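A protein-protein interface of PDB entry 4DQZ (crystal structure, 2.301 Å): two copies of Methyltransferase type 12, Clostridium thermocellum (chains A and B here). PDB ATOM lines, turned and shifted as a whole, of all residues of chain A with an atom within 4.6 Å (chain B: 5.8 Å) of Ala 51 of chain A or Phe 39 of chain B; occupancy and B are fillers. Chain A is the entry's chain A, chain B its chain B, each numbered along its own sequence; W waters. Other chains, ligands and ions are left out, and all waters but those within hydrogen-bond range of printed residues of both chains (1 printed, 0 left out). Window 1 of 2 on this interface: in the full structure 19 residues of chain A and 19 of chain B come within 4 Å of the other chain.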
ATOM      1  N   ILE A   2     -10.678   5.906 -26.645  1.00  0.00           N
ATOM      2  CA  ILE A   2     -10.805   4.509 -27.021  1.00  0.00           C
ATOM      3  C   ILE A   2     -12.175   4.232 -27.660  1.00  0.00           C
ATOM      4  O   ILE A   2     -13.179   4.822 -27.283  1.00  0.00           O
ATOM      5  CB  ILE A   2     -10.639   3.632 -25.788  1.00  0.00           C
ATOM      6  CG1 ILE A   2      -9.315   3.965 -25.073  1.00  0.00           C
ATOM      7  CG2 ILE A   2     -10.691   2.145 -26.153  1.00  0.00           C
ATOM      8  CD1 ILE A   2      -9.263   3.515 -23.605  1.00  0.00           C
ATOM      9  N   LEU A   3     -12.197   3.352 -28.644  1.00  0.00           N
ATOM     10  CA  LEU A   3     -13.447   2.889 -29.222  1.00  0.00           C
ATOM     11  C   LEU A   3     -13.528   1.381 -29.088  1.00  0.00           C
ATOM     12  O   LEU A   3     -12.604   0.674 -29.474  1.00  0.00           O
ATOM     13  CB  LEU A   3     -13.528   3.274 -30.697  1.00  0.00           C
ATOM     14  CG  LEU A   3     -14.670   2.621 -31.488  1.00  0.00           C
ATOM     15  CD1 LEU A   3     -15.970   3.215 -31.025  1.00  0.00           C
ATOM     16  CD2 LEU A   3     -14.489   2.838 -32.980  1.00  0.00           C
ATOM     17  N   THR A   4     -14.632   0.879 -28.557  1.00  0.00           N
ATOM     18  CA  THR A   4     -14.884  -0.565 -28.650  1.00  0.00           C
ATOM     19  C   THR A   4     -16.163  -0.875 -29.424  1.00  0.00           C
ATOM     20  O   THR A   4     -17.138  -0.110 -29.400  1.00  0.00           O
ATOM     21  CB  THR A   4     -14.993  -1.234 -27.255  1.00  0.00           C
ATOM     22  OG1 THR A   4     -16.197  -0.778 -26.625  1.00  0.00           O
ATOM     23  CG2 THR A   4     -13.752  -0.874 -26.364  1.00  0.00           C
ATOM     24  N   HIS A  37      -3.753   1.496 -31.628  1.00  0.00           N
ATOM     25  CA  HIS A  37      -3.621   0.072 -31.352  1.00  0.00           C
ATOM     26  C   HIS A  37      -5.002  -0.553 -31.552  1.00  0.00           C
ATOM     27  O   HIS A  37      -6.012   0.001 -31.126  1.00  0.00           O
ATOM     28  CB  HIS A  37      -3.189  -0.134 -29.896  1.00  0.00           C
ATOM     29  CG  HIS A  37      -1.947   0.609 -29.526  1.00  0.00           C
ATOM     30  ND1 HIS A  37      -0.688   0.185 -29.900  1.00  0.00           N
ATOM     31  CD2 HIS A  37      -1.767   1.743 -28.812  1.00  0.00           C
ATOM     32  CE1 HIS A  37       0.211   1.031 -29.432  1.00  0.00           C
ATOM     33  NE2 HIS A  37      -0.415   1.979 -28.761  1.00  0.00           N
ATOM     34  N   ILE A  38      -5.048  -1.690 -32.219  1.00  0.00           N
ATOM     35  CA  ILE A  38      -6.293  -2.406 -32.364  1.00  0.00           C
ATOM     36  C   ILE A  38      -6.111  -3.840 -31.904  1.00  0.00           C
ATOM     37  O   ILE A  38      -5.126  -4.488 -32.218  1.00  0.00           O
ATOM     38  CB  ILE A  38      -6.833  -2.371 -33.808  1.00  0.00           C
ATOM     39  CG1 ILE A  38      -8.031  -3.309 -33.943  1.00  0.00           C
ATOM     40  CG2 ILE A  38      -5.793  -2.821 -34.768  1.00  0.00           C
ATOM     41  CD1 ILE A  38      -8.766  -3.157 -35.216  1.00  0.00           C
ATOM     42  N   PHE A  39      -7.065  -4.330 -31.129  1.00  0.00           N
ATOM     43  CA  PHE A  39      -7.050  -5.733 -30.779  1.00  0.00           C
ATOM     44  C   PHE A  39      -8.451  -6.109 -30.370  1.00  0.00           C
ATOM     45  O   PHE A  39      -9.338  -5.259 -30.240  1.00  0.00           O
ATOM     46  CB  PHE A  39      -6.021  -6.038 -29.645  1.00  0.00           C
ATOM     47  CG  PHE A  39      -6.439  -5.529 -28.296  1.00  0.00           C
ATOM     48  CD1 PHE A  39      -6.437  -4.171 -28.019  1.00  0.00           C
ATOM     49  CD2 PHE A  39      -6.822  -6.406 -27.309  1.00  0.00           C
ATOM     50  CE1 PHE A  39      -6.818  -3.693 -26.780  1.00  0.00           C
ATOM     51  CE2 PHE A  39      -7.198  -5.937 -26.063  1.00  0.00           C
ATOM     52  CZ  PHE A  39      -7.202  -4.583 -25.799  1.00  0.00           C
ATOM     53  N   PRO A  41     -10.255  -7.802 -27.348  1.00  0.00           N
ATOM     54  CA  PRO A  41     -10.245  -8.390 -26.002  1.00  0.00           C
ATOM     55  C   PRO A  41     -11.056  -9.681 -25.922  1.00  0.00           C
ATOM     56  O   PRO A  41     -10.803 -10.513 -25.053  1.00  0.00           O
ATOM     57  CB  PRO A  41     -10.868  -7.290 -25.119  1.00  0.00           C
ATOM     58  CG  PRO A  41     -11.356  -6.220 -26.047  1.00  0.00           C
ATOM     59  CD  PRO A  41     -10.666  -6.388 -27.355  1.00  0.00           C
ATOM     60  N   THR A  49     -15.463  -8.543 -29.355  1.00  0.00           N
ATOM     61  CA  THR A  49     -15.275  -7.151 -29.027  1.00  0.00           C
ATOM     62  C   THR A  49     -13.962  -6.657 -29.596  1.00  0.00           C
ATOM     63  O   THR A  49     -12.923  -7.268 -29.392  1.00  0.00           O
ATOM     64  CB  THR A  49     -15.303  -6.926 -27.525  1.00  0.00           C
ATOM     65  OG1 THR A  49     -16.622  -7.170 -27.053  1.00  0.00           O
ATOM     66  CG2 THR A  49     -14.964  -5.464 -27.197  1.00  0.00           C
ATOM     67  N   VAL A  50     -14.023  -5.574 -30.354  1.00  0.00           N
ATOM     68  CA  VAL A  50     -12.819  -5.014 -30.922  1.00  0.00           C
ATOM     69  C   VAL A  50     -12.536  -3.756 -30.113  1.00  0.00           C
ATOM     70  O   VAL A  50     -13.459  -3.130 -29.621  1.00  0.00           O
ATOM     71  CB  VAL A  50     -12.959  -4.669 -32.415  1.00  0.00           C
ATOM     72  CG1 VAL A  50     -13.854  -3.429 -32.611  1.00  0.00           C
ATOM     73  CG2 VAL A  50     -11.576  -4.402 -33.018  1.00  0.00           C
ATOM     74  N   ALA A  51     -11.267  -3.422 -29.933  1.00  0.00           N
ATOM     75  CA  ALA A  51     -10.907  -2.158 -29.292  1.00  0.00           C
ATOM     76  C   ALA A  51      -9.924  -1.393 -30.149  1.00  0.00           C
ATOM     77  O   ALA A  51      -9.035  -1.958 -30.765  1.00  0.00           O
ATOM     78  CB  ALA A  51     -10.294  -2.380 -27.924  1.00  0.00           C
ATOM     79  N   LEU A  52     -10.076  -0.089 -30.175  1.00  0.00           N
ATOM     80  CA  LEU A  52      -9.122   0.728 -30.901  1.00  0.00           C
ATOM     81  C   LEU A  52      -8.693   1.839 -29.964  1.00  0.00           C
ATOM     82  O   LEU A  52      -9.479   2.682 -29.554  1.00  0.00           O
ATOM     83  CB  LEU A  52      -9.736   1.295 -32.169  1.00  0.00           C
ATOM     84  CG  LEU A  52      -8.899   2.318 -32.946  1.00  0.00           C
ATOM     85  CD1 LEU A  52      -7.656   1.691 -33.555  1.00  0.00           C
ATOM     86  CD2 LEU A  52      -9.747   2.961 -34.018  1.00  0.00           C
ATOM     87  N   LEU A  53      -7.430   1.813 -29.609  1.00  0.00           N
ATOM     88  CA  LEU A  53      -6.966   2.663 -28.535  1.00  0.00           C
ATOM     89  C   LEU A  53      -6.073   3.706 -29.182  1.00  0.00           C
ATOM     90  O   LEU A  53      -5.179   3.365 -29.955  1.00  0.00           O
ATOM     91  CB  LEU A  53      -6.242   1.804 -27.497  1.00  0.00           C
ATOM     92  CG  LEU A  53      -5.632   2.464 -26.267  1.00  0.00           C
ATOM     93  CD1 LEU A  53      -5.716   1.495 -25.079  1.00  0.00           C
ATOM     94  CD2 LEU A  53      -4.194   2.850 -26.561  1.00  0.00           C
ATOM     95  N   MET A 123     -14.724   5.923 -25.136  1.00  0.00           N
ATOM     96  CA  MET A 123     -14.221   6.363 -23.840  1.00  0.00           C
ATOM     97  C   MET A 123     -13.283   7.571 -23.944  1.00  0.00           C
ATOM     98  O   MET A 123     -12.421   7.630 -24.820  1.00  0.00           O
ATOM     99  CB  MET A 123     -13.500   5.205 -23.139  1.00  0.00           C
ATOM    100  CG  MET A 123     -14.162   3.868 -23.393  1.00  0.00           C
ATOM    101  SD  MET A 123     -13.298   2.454 -22.656  1.00  0.00           S
ATOM    102  CE  MET A 123     -13.322   2.840 -20.918  1.00  0.00           C
ATOM    103  N   PRO B  23     -12.759   1.356 -13.450  1.00  0.00           N
ATOM    104  CA  PRO B  23     -13.215   1.019 -14.800  1.00  0.00           C
ATOM    105  C   PRO B  23     -13.530   2.250 -15.647  1.00  0.00           C
ATOM    106  O   PRO B  23     -13.290   2.234 -16.856  1.00  0.00           O
ATOM    107  CB  PRO B  23     -14.490   0.210 -14.543  1.00  0.00           C
ATOM    108  CG  PRO B  23     -14.303  -0.367 -13.165  1.00  0.00           C
ATOM    109  CD  PRO B  23     -13.564   0.689 -12.408  1.00  0.00           C
ATOM    110  N   PRO B  26      -9.688   5.091 -17.963  1.00  0.00           N
ATOM    111  CA  PRO B  26      -8.491   4.627 -18.683  1.00  0.00           C
ATOM    112  C   PRO B  26      -7.268   5.407 -18.246  1.00  0.00           C
ATOM    113  O   PRO B  26      -7.381   6.568 -17.871  1.00  0.00           O
ATOM    114  CB  PRO B  26      -8.814   4.953 -20.133  1.00  0.00           C
ATOM    115  CG  PRO B  26     -10.341   4.879 -20.185  1.00  0.00           C
ATOM    116  CD  PRO B  26     -10.789   5.441 -18.870  1.00  0.00           C
ATOM    117  N   GLN B  27      -6.104   4.786 -18.292  1.00  0.00           N
ATOM    118  CA  GLN B  27      -4.931   5.435 -17.749  1.00  0.00           C
ATOM    119  C   GLN B  27      -3.681   4.938 -18.443  1.00  0.00           C
ATOM    120  O   GLN B  27      -3.614   3.787 -18.879  1.00  0.00           O
ATOM    121  CB  GLN B  27      -4.875   5.143 -16.260  1.00  0.00           C
ATOM    122  CG  GLN B  27      -4.008   6.034 -15.422  1.00  0.00           C
ATOM    123  CD  GLN B  27      -4.038   5.582 -13.976  1.00  0.00           C
ATOM    124  OE1 GLN B  27      -4.910   4.803 -13.583  1.00  0.00           O
ATOM    125  NE2 GLN B  27      -3.084   6.046 -13.185  1.00  0.00           N
ATOM    126  N   HIS B  37      -0.896   0.906 -21.169  1.00  0.00           N
ATOM    127  CA  HIS B  37      -2.239   1.470 -21.158  1.00  0.00           C
ATOM    128  C   HIS B  37      -3.135   0.472 -20.429  1.00  0.00           C
ATOM    129  O   HIS B  37      -3.040  -0.732 -20.650  1.00  0.00           O
ATOM    130  CB  HIS B  37      -2.741   1.624 -22.597  1.00  0.00           C
ATOM    131  CG  HIS B  37      -1.826   2.417 -23.472  1.00  0.00           C
ATOM    132  ND1 HIS B  37      -1.745   3.793 -23.407  1.00  0.00           N
ATOM    133  CD2 HIS B  37      -0.960   2.032 -24.436  1.00  0.00           C
ATOM    134  CE1 HIS B  37      -0.863   4.216 -24.292  1.00  0.00           C
ATOM    135  NE2 HIS B  37      -0.380   3.171 -24.936  1.00  0.00           N
ATOM    136  N   ILE B  38      -3.985   0.966 -19.548  1.00  0.00           N
ATOM    137  CA  ILE B  38      -4.943   0.110 -18.888  1.00  0.00           C
ATOM    138  C   ILE B  38      -6.342   0.675 -19.060  1.00  0.00           C
ATOM    139  O   ILE B  38      -6.568   1.865 -18.921  1.00  0.00           O
ATOM    140  CB  ILE B  38      -4.625  -0.087 -17.391  1.00  0.00           C
ATOM    141  CG1 ILE B  38      -5.776  -0.824 -16.707  1.00  0.00           C
ATOM    142  CG2 ILE B  38      -4.468   1.224 -16.718  1.00  0.00           C
ATOM    143  CD1 ILE B  38      -5.469  -1.266 -15.338  1.00  0.00           C
ATOM    144  N   PHE B  39      -7.287  -0.188 -19.392  1.00  0.00           N
ATOM    145  CA  PHE B  39      -8.667   0.245 -19.424  1.00  0.00           C
ATOM    146  C   PHE B  39      -9.524  -0.988 -19.310  1.00  0.00           C
ATOM    147  O   PHE B  39      -9.034  -2.122 -19.347  1.00  0.00           O
ATOM    148  CB  PHE B  39      -8.995   1.048 -20.718  1.00  0.00           C
ATOM    149  CG  PHE B  39      -9.054   0.201 -21.961  1.00  0.00           C
ATOM    150  CD1 PHE B  39      -7.899  -0.329 -22.513  1.00  0.00           C
ATOM    151  CD2 PHE B  39     -10.259  -0.053 -22.577  1.00  0.00           C
ATOM    152  CE1 PHE B  39      -7.943  -1.106 -23.653  1.00  0.00           C
ATOM    153  CE2 PHE B  39     -10.312  -0.827 -23.729  1.00  0.00           C
ATOM    154  CZ  PHE B  39      -9.157  -1.356 -24.259  1.00  0.00           C
ATOM    155  N   TYR B  40     -10.815  -0.756 -19.135  1.00  0.00           N
ATOM    156  CA  TYR B  40     -11.763  -1.834 -19.055  1.00  0.00           C
ATOM    157  C   TYR B  40     -12.685  -1.787 -20.263  1.00  0.00           C
ATOM    158  O   TYR B  40     -13.575  -0.949 -20.338  1.00  0.00           O
ATOM    159  CB  TYR B  40     -12.597  -1.723 -17.788  1.00  0.00           C
ATOM    160  CG  TYR B  40     -11.877  -1.974 -16.498  1.00  0.00           C
ATOM    161  CD1 TYR B  40     -10.901  -1.092 -16.030  1.00  0.00           C
ATOM    162  CD2 TYR B  40     -12.207  -3.085 -15.710  1.00  0.00           C
ATOM    163  CE1 TYR B  40     -10.263  -1.331 -14.798  1.00  0.00           C
ATOM    164  CE2 TYR B  40     -11.588  -3.317 -14.509  1.00  0.00           C
ATOM    165  CZ  TYR B  40     -10.624  -2.440 -14.054  1.00  0.00           C
ATOM    166  OH  TYR B  40     -10.033  -2.693 -12.842  1.00  0.00           O
ATOM    167  N   PRO B  41     -12.470  -2.690 -21.218  1.00  0.00           N
ATOM    168  CA  PRO B  41     -13.407  -2.762 -22.344  1.00  0.00           C
ATOM    169  C   PRO B  41     -14.839  -3.065 -21.904  1.00  0.00           C
ATOM    170  O   PRO B  41     -15.783  -2.724 -22.614  1.00  0.00           O
ATOM    171  CB  PRO B  41     -12.841  -3.901 -23.213  1.00  0.00           C
ATOM    172  CG  PRO B  41     -11.733  -4.526 -22.428  1.00  0.00           C
ATOM    173  CD  PRO B  41     -11.294  -3.561 -21.392  1.00  0.00           C
ATOM    174  N   THR B  49     -14.003  -6.760 -17.639  1.00  0.00           N
ATOM    175  CA  THR B  49     -12.777  -7.145 -18.293  1.00  0.00           C
ATOM    176  C   THR B  49     -11.795  -5.994 -18.259  1.00  0.00           C
ATOM    177  O   THR B  49     -12.132  -4.877 -18.624  1.00  0.00           O
ATOM    178  CB  THR B  49     -13.026  -7.566 -19.730  1.00  0.00           C
ATOM    179  OG1 THR B  49     -13.750  -8.791 -19.723  1.00  0.00           O
ATOM    180  CG2 THR B  49     -11.693  -7.833 -20.444  1.00  0.00           C
ATOM    181  N   VAL B  50     -10.595  -6.261 -17.768  1.00  0.00           N
ATOM    182  CA  VAL B  50      -9.576  -5.243 -17.723  1.00  0.00           C
ATOM    183  C   VAL B  50      -8.590  -5.597 -18.829  1.00  0.00           C
ATOM    184  O   VAL B  50      -8.421  -6.763 -19.140  1.00  0.00           O
ATOM    185  CB  VAL B  50      -8.851  -5.173 -16.368  1.00  0.00           C
ATOM    186  CG1 VAL B  50      -7.900  -6.372 -16.186  1.00  0.00           C
ATOM    187  CG2 VAL B  50      -8.047  -3.869 -16.274  1.00  0.00           C
ATOM    188  N   ALA B  51      -7.982  -4.593 -19.448  1.00  0.00           N
ATOM    189  CA  ALA B  51      -6.927  -4.851 -20.423  1.00  0.00           C
ATOM    190  C   ALA B  51      -5.696  -4.038 -20.084  1.00  0.00           C
ATOM    191  O   ALA B  51      -5.783  -2.897 -19.667  1.00  0.00           O
ATOM    192  CB  ALA B  51      -7.366  -4.503 -21.832  1.00  0.00           C
ATOM    193  N   LEU B  52      -4.540  -4.627 -20.287  1.00  0.00           N
ATOM    194  CA  LEU B  52      -3.318  -3.880 -20.075  1.00  0.00           C
ATOM    195  C   LEU B  52      -2.475  -4.081 -21.313  1.00  0.00           C
ATOM    196  O   LEU B  52      -2.056  -5.183 -21.638  1.00  0.00           O
ATOM    197  CB  LEU B  52      -2.589  -4.368 -18.838  1.00  0.00           C
ATOM    198  CG  LEU B  52      -1.185  -3.800 -18.589  1.00  0.00           C
ATOM    199  CD1 LEU B  52      -1.219  -2.314 -18.265  1.00  0.00           C
ATOM    200  CD2 LEU B  52      -0.526  -4.569 -17.472  1.00  0.00           C
ATOM    201  N   LEU B  53      -2.244  -2.993 -22.014  1.00  0.00           N
ATOM    202  CA  LEU B  53      -1.656  -3.092 -23.332  1.00  0.00           C
ATOM    203  C   LEU B  53      -0.259  -2.504 -23.219  1.00  0.00           C
ATOM    204  O   LEU B  53      -0.085  -1.406 -22.690  1.00  0.00           O
ATOM    205  CB  LEU B  53      -2.548  -2.353 -24.331  1.00  0.00           C
ATOM    206  CG  LEU B  53      -2.144  -2.288 -25.799  1.00  0.00           C
ATOM    207  CD1 LEU B  53      -3.403  -2.277 -26.670  1.00  0.00           C
ATOM    208  CD2 LEU B  53      -1.305  -1.045 -26.036  1.00  0.00           C
HETATM  209  O   HOH W   1       0.746   3.382 -27.132  1.00  0.00           O
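Among the printed residues, merely in contact across the chains: Met 123 of chain A with Pro 26 of chain B (3.7 Å), Phe 39 of chain A with Leu 53 of chain B (3.7 Å), Ile 2 of chain A with Phe 39 of chain B (3.7 Å), Leu 53 of chain A with Phe 39 of chain B (3.7 Å), Ile 2 of chain A with Pro 26 of chain B (3.8 Å), Met 123 of chain A with Tyr 40 of chain B (3.8 Å), Leu 53 of chain A with His 37 of chain B (3.9 Å), His 37 of chain A with Leu 53 of chain B (3.9 Å), Met 123 of chain A with Phe 39 of chain B (3.9 Å), Pro 41 of chain A with Pro 41 of chain B (3.95 Å), Phe 39 of chain A with Ala 51 of chain B (3.97 Å) and Ala 51 of chain A with Phe 39 of chain B (3.97 Å).
His 37 of chain A touches Leu 53 of chain B, and with the chains exchanged Leu 53 of chain A touches His 37 of chain B.
Phe 39 of chain A touches Ala 51 of chain B, and with the chains exchanged Ala 51 of chain A touches Phe 39 of chain B.
Phe 39 of chain A touches Leu 53 of chain B, and with the chains exchanged Leu 53 of chain A touches Phe 39 of chain B.
Pro 41 of chain A touches its own counterpart, Pro 41 of chain B.
9 positions are printed for both chains.
Of the 12 pairs that touch across the chains among the printed residues, 7 have their exchanged pair printed and touching as well.
Of chain B, only Phe 39 comes within 4 Å of Ala 51 of chain A.
Of chain A, only Ile 2 (3.7 Å), Ala 51 (3.97 Å), Leu 53 (3.7 Å) and Met 123 (3.9 Å) come within 4 Å of Phe 39 of chain B.
Of the printed residues of chain A, Leu 53 of chain B touches His 37 and Phe 39.
Of the printed residues of chain B, Ile 2 of chain A touches Pro 26 (3.8 Å) and Phe 39 (3.7 Å).
Printed residues of chain A within 4 Å of Pro 26 of chain B: Ile 2 and Met 123.
Printed residues of chain B within 4 Å of Pro 41 of chain A: Pro 41 (3.95 Å).
The nearest printed residue of chain A that does not touch Pro 41 of chain B is Thr 4 of chain A (4.5 Å).
Water W1 lies within hydrogen-bond range of a ring nitrogen (NE2) of His 37 of chain A and a ring nitrogen (NE2) of His 37 of chain B.
The backbone carbonyl oxygen (O) of Ile 2 of chain A lies within hydrogen-bond range of the backbone NH (N) of Met 123 of chain A (2.9 Å).
The backbone NH (N) of Leu 53 of chain A lies within hydrogen-bond range of the backbone carbonyl oxygen (O) of His 37 of chain A (2.8 Å).
The backbone carbonyl oxygen (O) of Phe 39 of chain A is in hydrogen-bond range of the backbone NH (N) of Ala 51 of chain A.
The backbone carbonyl oxygen (O) of His 37 of chain B is in hydrogen-bond range of the backbone NH (N) of Leu 53 of chain B (2.8 Å).
O of Phe 39 of chain B lies within hydrogen-bond range of N of Ala 51 of chain B.
Hydrophobic or aromatic side chains of chain A that line the printed part of chain B: Ile 2, His 37, Phe 39, Pro 41, Ala 51, Leu 53 and Met 123.
Among the printed residues, 12 pairs touch across the chains.
Among the printed residues, no Asp or Glu carboxylate lies within 4 Å of a Lys or Arg side-chain nitrogen of the other chain.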
